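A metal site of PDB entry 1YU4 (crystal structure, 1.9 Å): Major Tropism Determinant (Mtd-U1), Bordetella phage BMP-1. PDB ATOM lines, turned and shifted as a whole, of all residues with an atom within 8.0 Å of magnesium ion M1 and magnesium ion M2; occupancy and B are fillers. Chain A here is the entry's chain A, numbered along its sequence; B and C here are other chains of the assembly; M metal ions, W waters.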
ATOM      1  N   ASN A 254     -10.715  15.836  20.421  1.00  0.00           N
ATOM      2  CA  ASN A 254     -11.041  14.638  19.683  1.00  0.00           C
ATOM      3  C   ASN A 254     -12.554  14.544  19.602  1.00  0.00           C
ATOM      4  O   ASN A 254     -13.266  15.414  20.099  1.00  0.00           O
ATOM      5  CB  ASN A 254     -10.414  13.405  20.343  1.00  0.00           C
ATOM      6  CG  ASN A 254      -9.898  12.392  19.323  1.00  0.00           C
ATOM      7  OD1 ASN A 254     -10.651  11.899  18.481  1.00  0.00           O
ATOM      8  ND2 ASN A 254      -8.620  12.078  19.400  1.00  0.00           N
ATOM      9  N   ASN A 311      -8.000  16.852  16.974  1.00  0.00           N
ATOM     10  CA  ASN A 311      -6.717  16.188  17.234  1.00  0.00           C
ATOM     11  C   ASN A 311      -6.793  14.697  16.876  1.00  0.00           C
ATOM     12  O   ASN A 311      -6.411  13.828  17.653  1.00  0.00           O
ATOM     13  CB  ASN A 311      -6.307  16.407  18.700  1.00  0.00           C
ATOM     14  CG  ASN A 311      -4.865  16.055  18.967  1.00  0.00           C
ATOM     15  OD1 ASN A 311      -3.947  16.526  18.274  1.00  0.00           O
ATOM     16  ND2 ASN A 311      -4.649  15.229  19.995  1.00  0.00           N
ATOM     17  N   GLU A 312      -7.290  14.433  15.673  1.00  0.00           N
ATOM     18  CA  GLU A 312      -7.501  13.068  15.212  1.00  0.00           C
ATOM     19  C   GLU A 312      -7.487  13.051  13.695  1.00  0.00           C
ATOM     20  O   GLU A 312      -8.018  13.947  13.038  1.00  0.00           O
ATOM     21  CB  GLU A 312      -8.838  12.546  15.751  1.00  0.00           C
ATOM     22  CG  GLU A 312      -9.227  11.135  15.304  1.00  0.00           C
ATOM     23  CD  GLU A 312      -8.301  10.062  15.827  1.00  0.00           C
ATOM     24  OE1 GLU A 312      -7.609  10.289  16.840  1.00  0.00           O
ATOM     25  OE2 GLU A 312      -8.257   8.980  15.228  1.00  0.00           O
ATOM     26  N   PHE A 313      -6.881  11.997  13.150  1.00  0.00           N
ATOM     27  CA  PHE A 313      -6.705  11.845  11.715  1.00  0.00           C
ATOM     28  C   PHE A 313      -7.415  10.594  11.206  1.00  0.00           C
ATOM     29  O   PHE A 313      -7.505   9.573  11.901  1.00  0.00           O
ATOM     30  CB  PHE A 313      -5.213  11.782  11.392  1.00  0.00           C
ATOM     31  CG  PHE A 313      -4.499  13.074  11.617  1.00  0.00           C
ATOM     32  CD1 PHE A 313      -4.309  13.961  10.569  1.00  0.00           C
ATOM     33  CD2 PHE A 313      -4.047  13.427  12.881  1.00  0.00           C
ATOM     34  CE1 PHE A 313      -3.664  15.171  10.767  1.00  0.00           C
ATOM     35  CE2 PHE A 313      -3.409  14.639  13.091  1.00  0.00           C
ATOM     36  CZ  PHE A 313      -3.217  15.513  12.038  1.00  0.00           C
ATOM     37  N   GLY A 314      -7.916  10.690   9.975  1.00  0.00           N
ATOM     38  CA  GLY A 314      -8.638   9.620   9.317  1.00  0.00           C
ATOM     39  C   GLY A 314      -9.458  10.157   8.160  1.00  0.00           C
ATOM     40  O   GLY A 314      -9.482  11.369   7.905  1.00  0.00           O
ATOM     41  N   GLY A 315     -10.159   9.275   7.469  1.00  0.00           N
ATOM     42  CA  GLY A 315     -10.975   9.670   6.341  1.00  0.00           C
ATOM     43  C   GLY A 315     -10.199   9.697   5.036  1.00  0.00           C
ATOM     44  O   GLY A 315      -9.386   8.809   4.762  1.00  0.00           O
ATOM     45  N   PRO A 336      -3.673  11.425   5.871  1.00  0.00           N
ATOM     46  CA  PRO A 336      -5.106  11.461   6.177  1.00  0.00           C
ATOM     47  C   PRO A 336      -5.595  12.852   6.563  1.00  0.00           C
ATOM     48  O   PRO A 336      -4.829  13.681   7.092  1.00  0.00           O
ATOM     49  CB  PRO A 336      -5.226  10.500   7.357  1.00  0.00           C
ATOM     50  CG  PRO A 336      -3.910  10.533   7.997  1.00  0.00           C
ATOM     51  CD  PRO A 336      -2.922  10.666   6.880  1.00  0.00           C
ATOM     52  N   ALA A 337      -6.877  13.090   6.322  1.00  0.00           N
ATOM     53  CA  ALA A 337      -7.528  14.310   6.775  1.00  0.00           C
ATOM     54  C   ALA A 337      -7.391  14.458   8.282  1.00  0.00           C
ATOM     55  O   ALA A 337      -7.303  13.470   9.014  1.00  0.00           O
ATOM     56  CB  ALA A 337      -9.016  14.308   6.392  1.00  0.00           C
ATOM     57  N   TRP A 358     -14.225  14.721   7.335  1.00  0.00           N
ATOM     58  CA  TRP A 358     -12.889  14.118   7.271  1.00  0.00           C
ATOM     59  C   TRP A 358     -12.379  14.124   5.843  1.00  0.00           C
ATOM     60  O   TRP A 358     -11.795  13.143   5.377  1.00  0.00           O
ATOM     61  CB  TRP A 358     -12.908  12.686   7.807  1.00  0.00           C
ATOM     62  CG  TRP A 358     -13.534  12.523   9.151  1.00  0.00           C
ATOM     63  CD1 TRP A 358     -14.863  12.576   9.456  1.00  0.00           C
ATOM     64  CD2 TRP A 358     -12.860  12.207  10.371  1.00  0.00           C
ATOM     65  NE1 TRP A 358     -15.052  12.324  10.786  1.00  0.00           N
ATOM     66  CE2 TRP A 358     -13.844  12.087  11.379  1.00  0.00           C
ATOM     67  CE3 TRP A 358     -11.519  12.001  10.724  1.00  0.00           C
ATOM     68  CZ2 TRP A 358     -13.529  11.782  12.700  1.00  0.00           C
ATOM     69  CZ3 TRP A 358     -11.219  11.696  12.036  1.00  0.00           C
ATOM     70  CH2 TRP A 358     -12.217  11.592  13.014  1.00  0.00           C
ATOM     71  N   ASN B 254       1.916  11.833  19.094  1.00  0.00           N
ATOM     72  CA  ASN B 254       0.975  12.154  18.045  1.00  0.00           C
ATOM     73  C   ASN B 254       1.552  13.290  17.199  1.00  0.00           C
ATOM     74  O   ASN B 254       2.637  13.786  17.494  1.00  0.00           O
ATOM     75  CB  ASN B 254      -0.389  12.532  18.629  1.00  0.00           C
ATOM     76  CG  ASN B 254      -1.531  12.016  17.796  1.00  0.00           C
ATOM     77  OD1 ASN B 254      -1.621  12.317  16.616  1.00  0.00           O
ATOM     78  ND2 ASN B 254      -2.408  11.224  18.401  1.00  0.00           N
ATOM     79  N   ASN B 311       1.509   7.602  17.771  1.00  0.00           N
ATOM     80  CA  ASN B 311       0.382   7.026  18.491  1.00  0.00           C
ATOM     81  C   ASN B 311      -0.937   7.456  17.836  1.00  0.00           C
ATOM     82  O   ASN B 311      -1.814   8.026  18.490  1.00  0.00           O
ATOM     83  CB  ASN B 311       0.423   7.471  19.959  1.00  0.00           C
ATOM     84  CG  ASN B 311      -0.557   6.709  20.824  1.00  0.00           C
ATOM     85  OD1 ASN B 311      -0.584   5.478  20.801  1.00  0.00           O
ATOM     86  ND2 ASN B 311      -1.380   7.433  21.572  1.00  0.00           N
ATOM     87  N   GLU B 312      -1.050   7.189  16.547  1.00  0.00           N
ATOM     88  CA  GLU B 312      -2.173   7.651  15.745  1.00  0.00           C
ATOM     89  C   GLU B 312      -2.247   6.820  14.474  1.00  0.00           C
ATOM     90  O   GLU B 312      -1.220   6.472  13.876  1.00  0.00           O
ATOM     91  CB  GLU B 312      -2.001   9.137  15.399  1.00  0.00           C
ATOM     92  CG  GLU B 312      -3.080   9.760  14.530  1.00  0.00           C
ATOM     93  CD  GLU B 312      -4.463   9.780  15.144  1.00  0.00           C
ATOM     94  OE1 GLU B 312      -4.598   9.773  16.395  1.00  0.00           O
ATOM     95  OE2 GLU B 312      -5.440   9.797  14.373  1.00  0.00           O
ATOM     96  N   PHE B 313      -3.467   6.488  14.078  1.00  0.00           N
ATOM     97  CA  PHE B 313      -3.712   5.645  12.916  1.00  0.00           C
ATOM     98  C   PHE B 313      -4.521   6.384  11.846  1.00  0.00           C
ATOM     99  O   PHE B 313      -5.343   7.234  12.153  1.00  0.00           O
ATOM    100  CB  PHE B 313      -4.414   4.355  13.348  1.00  0.00           C
ATOM    101  CG  PHE B 313      -3.554   3.458  14.198  1.00  0.00           C
ATOM    102  CD1 PHE B 313      -2.870   2.388  13.639  1.00  0.00           C
ATOM    103  CD2 PHE B 313      -3.419   3.695  15.556  1.00  0.00           C
ATOM    104  CE1 PHE B 313      -2.065   1.552  14.419  1.00  0.00           C
ATOM    105  CE2 PHE B 313      -2.612   2.868  16.354  1.00  0.00           C
ATOM    106  CZ  PHE B 313      -1.942   1.799  15.785  1.00  0.00           C
ATOM    107  N   GLY B 314      -4.265   6.016  10.593  1.00  0.00           N
ATOM    108  CA  GLY B 314      -4.865   6.651   9.434  1.00  0.00           C
ATOM    109  C   GLY B 314      -3.996   6.420   8.206  1.00  0.00           C
ATOM    110  O   GLY B 314      -2.915   5.831   8.295  1.00  0.00           O
ATOM    111  N   GLY B 315      -4.475   6.877   7.055  1.00  0.00           N
ATOM    112  CA  GLY B 315      -3.762   6.691   5.802  1.00  0.00           C
ATOM    113  C   GLY B 315      -4.107   5.390   5.098  1.00  0.00           C
ATOM    114  O   GLY B 315      -5.279   5.003   5.032  1.00  0.00           O
ATOM    115  N   PRO B 336      -5.557   0.282   9.487  1.00  0.00           N
ATOM    116  CA  PRO B 336      -4.872   1.484   9.012  1.00  0.00           C
ATOM    117  C   PRO B 336      -3.403   1.516   9.404  1.00  0.00           C
ATOM    118  O   PRO B 336      -2.994   0.890  10.392  1.00  0.00           O
ATOM    119  CB  PRO B 336      -5.619   2.613   9.719  1.00  0.00           C
ATOM    120  CG  PRO B 336      -6.156   1.976  10.958  1.00  0.00           C
ATOM    121  CD  PRO B 336      -6.527   0.598  10.537  1.00  0.00           C
ATOM    122  N   ALA B 337      -2.633   2.282   8.646  1.00  0.00           N
ATOM    123  CA  ALA B 337      -1.241   2.538   8.977  1.00  0.00           C
ATOM    124  C   ALA B 337      -1.147   3.254  10.319  1.00  0.00           C
ATOM    125  O   ALA B 337      -2.057   3.989  10.709  1.00  0.00           O
ATOM    126  CB  ALA B 337      -0.596   3.399   7.902  1.00  0.00           C
ATOM    127  N   TRP B 358       2.181   7.719   6.164  1.00  0.00           N
ATOM    128  CA  TRP B 358       1.046   6.921   6.615  1.00  0.00           C
ATOM    129  C   TRP B 358       0.824   5.727   5.690  1.00  0.00           C
ATOM    130  O   TRP B 358      -0.318   5.373   5.375  1.00  0.00           O
ATOM    131  CB  TRP B 358      -0.220   7.767   6.713  1.00  0.00           C
ATOM    132  CG  TRP B 358      -0.090   9.053   7.489  1.00  0.00           C
ATOM    133  CD1 TRP B 358       0.512  10.209   7.084  1.00  0.00           C
ATOM    134  CD2 TRP B 358      -0.620   9.331   8.793  1.00  0.00           C
ATOM    135  NE1 TRP B 358       0.402  11.182   8.046  1.00  0.00           N
ATOM    136  CE2 TRP B 358      -0.290  10.664   9.107  1.00  0.00           C
ATOM    137  CE3 TRP B 358      -1.348   8.583   9.730  1.00  0.00           C
ATOM    138  CZ2 TRP B 358      -0.653  11.259  10.313  1.00  0.00           C
ATOM    139  CZ3 TRP B 358      -1.716   9.181  10.924  1.00  0.00           C
ATOM    140  CH2 TRP B 358      -1.364  10.510  11.202  1.00  0.00           C
ATOM    141  N   ASN C 254      -7.366   3.368  23.374  1.00  0.00           N
ATOM    142  CA  ASN C 254      -6.665   3.382  22.098  1.00  0.00           C
ATOM    143  C   ASN C 254      -5.920   2.044  21.944  1.00  0.00           C
ATOM    144  O   ASN C 254      -5.966   1.210  22.842  1.00  0.00           O
ATOM    145  CB  ASN C 254      -5.715   4.565  22.006  1.00  0.00           C
ATOM    146  CG  ASN C 254      -5.671   5.140  20.618  1.00  0.00           C
ATOM    147  OD1 ASN C 254      -5.390   4.433  19.653  1.00  0.00           O
ATOM    148  ND2 ASN C 254      -5.977   6.429  20.498  1.00  0.00           N
ATOM    149  N   ASN C 311     -11.040   4.561  21.147  1.00  0.00           N
ATOM    150  CA  ASN C 311     -11.007   6.020  21.027  1.00  0.00           C
ATOM    151  C   ASN C 311     -10.060   6.460  19.914  1.00  0.00           C
ATOM    152  O   ASN C 311      -9.203   7.312  20.099  1.00  0.00           O
ATOM    153  CB  ASN C 311     -10.588   6.651  22.356  1.00  0.00           C
ATOM    154  CG  ASN C 311     -10.896   8.141  22.415  1.00  0.00           C
ATOM    155  OD1 ASN C 311     -11.996   8.579  22.066  1.00  0.00           O
ATOM    156  ND2 ASN C 311      -9.926   8.935  22.854  1.00  0.00           N
ATOM    157  N   GLU C 312     -10.227   5.857  18.741  1.00  0.00           N
ATOM    158  CA  GLU C 312      -9.342   6.074  17.605  1.00  0.00           C
ATOM    159  C   GLU C 312     -10.068   5.754  16.316  1.00  0.00           C
ATOM    160  O   GLU C 312     -10.864   4.807  16.251  1.00  0.00           O
ATOM    161  CB  GLU C 312      -8.092   5.189  17.757  1.00  0.00           C
ATOM    162  CG  GLU C 312      -7.097   5.274  16.608  1.00  0.00           C
ATOM    163  CD  GLU C 312      -6.439   6.636  16.463  1.00  0.00           C
ATOM    164  OE1 GLU C 312      -6.388   7.416  17.435  1.00  0.00           O
ATOM    165  OE2 GLU C 312      -5.959   6.929  15.355  1.00  0.00           O
ATOM    166  N   PHE C 313      -9.806   6.559  15.301  1.00  0.00           N
ATOM    167  CA  PHE C 313     -10.507   6.463  14.027  1.00  0.00           C
ATOM    168  C   PHE C 313      -9.549   6.182  12.881  1.00  0.00           C
ATOM    169  O   PHE C 313      -8.424   6.690  12.867  1.00  0.00           O
ATOM    170  CB  PHE C 313     -11.282   7.755  13.766  1.00  0.00           C
ATOM    171  CG  PHE C 313     -12.477   7.915  14.668  1.00  0.00           C
ATOM    172  CD1 PHE C 313     -13.738   7.495  14.256  1.00  0.00           C
ATOM    173  CD2 PHE C 313     -12.336   8.486  15.930  1.00  0.00           C
ATOM    174  CE1 PHE C 313     -14.824   7.630  15.088  1.00  0.00           C
ATOM    175  CE2 PHE C 313     -13.431   8.617  16.765  1.00  0.00           C
ATOM    176  CZ  PHE C 313     -14.670   8.196  16.351  1.00  0.00           C
ATOM    177  N   GLY C 314      -9.997   5.362  11.939  1.00  0.00           N
ATOM    178  CA  GLY C 314      -9.239   5.044  10.749  1.00  0.00           C
ATOM    179  C   GLY C 314      -9.811   3.828  10.055  1.00  0.00           C
ATOM    180  O   GLY C 314     -10.821   3.289  10.489  1.00  0.00           O
ATOM    181  N   GLY C 315      -9.171   3.364   8.992  1.00  0.00           N
ATOM    182  CA  GLY C 315      -9.643   2.202   8.255  1.00  0.00           C
ATOM    183  C   GLY C 315     -10.680   2.567   7.197  1.00  0.00           C
ATOM    184  O   GLY C 315     -10.531   3.539   6.462  1.00  0.00           O
ATOM    185  N   PRO C 336     -14.499   8.017   9.062  1.00  0.00           N
ATOM    186  CA  PRO C 336     -13.720   6.787   9.268  1.00  0.00           C
ATOM    187  C   PRO C 336     -14.349   5.861  10.317  1.00  0.00           C
ATOM    188  O   PRO C 336     -15.043   6.320  11.243  1.00  0.00           O
ATOM    189  CB  PRO C 336     -12.370   7.312   9.760  1.00  0.00           C
ATOM    190  CG  PRO C 336     -12.693   8.640  10.384  1.00  0.00           C
ATOM    191  CD  PRO C 336     -13.779   9.207   9.533  1.00  0.00           C
ATOM    192  N   ALA C 337     -14.090   4.567  10.185  1.00  0.00           N
ATOM    193  CA  ALA C 337     -14.457   3.612  11.225  1.00  0.00           C
ATOM    194  C   ALA C 337     -13.875   4.038  12.559  1.00  0.00           C
ATOM    195  O   ALA C 337     -12.847   4.703  12.625  1.00  0.00           O
ATOM    196  CB  ALA C 337     -13.976   2.207  10.870  1.00  0.00           C
ATOM    197  N   TRP C 358     -11.398  -2.471  11.731  1.00  0.00           N
ATOM    198  CA  TRP C 358     -11.566  -1.057  11.389  1.00  0.00           C
ATOM    199  C   TRP C 358     -12.589  -0.905  10.247  1.00  0.00           C
ATOM    200  O   TRP C 358     -12.427  -0.083   9.351  1.00  0.00           O
ATOM    201  CB  TRP C 358     -10.231  -0.437  11.015  1.00  0.00           C
ATOM    202  CG  TRP C 358      -9.164  -0.550  12.063  1.00  0.00           C
ATOM    203  CD1 TRP C 358      -8.435  -1.680  12.359  1.00  0.00           C
ATOM    204  CD2 TRP C 358      -8.674   0.483  12.921  1.00  0.00           C
ATOM    205  NE1 TRP C 358      -7.541  -1.404  13.364  1.00  0.00           N
ATOM    206  CE2 TRP C 358      -7.651  -0.083  13.711  1.00  0.00           C
ATOM    207  CE3 TRP C 358      -8.996   1.838  13.098  1.00  0.00           C
ATOM    208  CZ2 TRP C 358      -6.947   0.657  14.670  1.00  0.00           C
ATOM    209  CZ3 TRP C 358      -8.293   2.573  14.048  1.00  0.00           C
ATOM    210  CH2 TRP C 358      -7.284   1.971  14.826  1.00  0.00           C
HETATM  211 MG    MG M   1      -5.952   9.446  17.915  1.00  0.00          MG
HETATM  212 MG    MG M   2      -6.839   8.193  13.577  1.00  0.00          MG
HETATM  213  O   HOH W   1      -4.363   8.829  19.165  1.00  0.00           O
HETATM  214  O   HOH W   2      -7.293   9.098  19.694  1.00  0.00           O
HETATM  215  O   HOH W   3      -5.660  11.410  18.598  1.00  0.00           O
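The side-chain carboxylate (OE1) of Glu 312 of chain B sits close to the side-chain amide nitrogen (ND2) of Asn 254 of chain B, 3.3 Å away. The side-chain amide nitrogen (ND2) of Asn 254 of chain C sits close to the side-chain carboxylate (OE1) of Glu 312 of chain C, 3.2 Å away. The side-chain carboxylate of Glu 312 of chain A sits close to the side-chain amide nitrogen of Asn 254 of chain A, 3.3 Å away. O of Asn 311 of chain C is in hydrogen-bond range of ND2 of Asn 254 of chain C (3.4 Å). The side-chain amide nitrogen (ND2) of Asn 254 of chain B is in hydrogen-bond range of the backbone carbonyl oxygen (O) of Asn 311 of chain B.
Asn 254 of chain B touches magnesium ion M1. ND2 of Asn 254 of chain C touches magnesium ion M1 (3.97 Å). Five residues have an atom within 4 Å of magnesium ion M1: Glu 312 of chain A, Asn 254 of chain B, Glu 312 of chain B, Asn 254 of chain C and Glu 312 of chain C.
The nearest printed residue that does not touch magnesium ion M2 is Gly 314 of chain B (4.5 Å).
Magnesium ion M1 is bound by OE1 of Glu 312 of chain B (2.1 Å), water W3 (2.1 Å), water W1 (2.1 Å), OE1 of Glu 312 of chain C (2.1 Å), OE1 of Glu 312 of chain A (2.1 Å) and water W2 (2.3 Å). Magnesium ion M1 has six donor atoms within binding distance.
Magnesium ion M2 is bound by the backbone carbonyl oxygen of Phe 313 of chain A (2.3 Å), the side-chain carboxylate of Glu 312 of chain B (2.3 Å), the backbone carbonyl oxygen of Phe 313 of chain B (2.3 Å), the backbone carbonyl oxygen of Phe 313 of chain C (2.3 Å), the side-chain carboxylate of Glu 312 of chain A (2.3 Å) and the side-chain carboxylate of Glu 312 of chain C (2.4 Å).
Water W1 lies within hydrogen-bond range of the backbone carbonyl oxygen (O) of Asn 311 of chain B (2.8 Å), the side-chain amide nitrogen (ND2) of Asn 254 of chain C (3.2 Å) and the side-chain amide nitrogen (ND2) of Asn 254 of chain B (3.2 Å). Water W3 lies within hydrogen-bond range of O of Asn 311 of chain A (2.7 Å), ND2 of Asn 254 of chain A (3.1 Å) and ND2 of Asn 254 of chain B (3.3 Å). Water W2 lies within hydrogen-bond range of O of Asn 311 of chain C, ND2 of Asn 254 of chain C and ND2 of Asn 254 of chain A.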
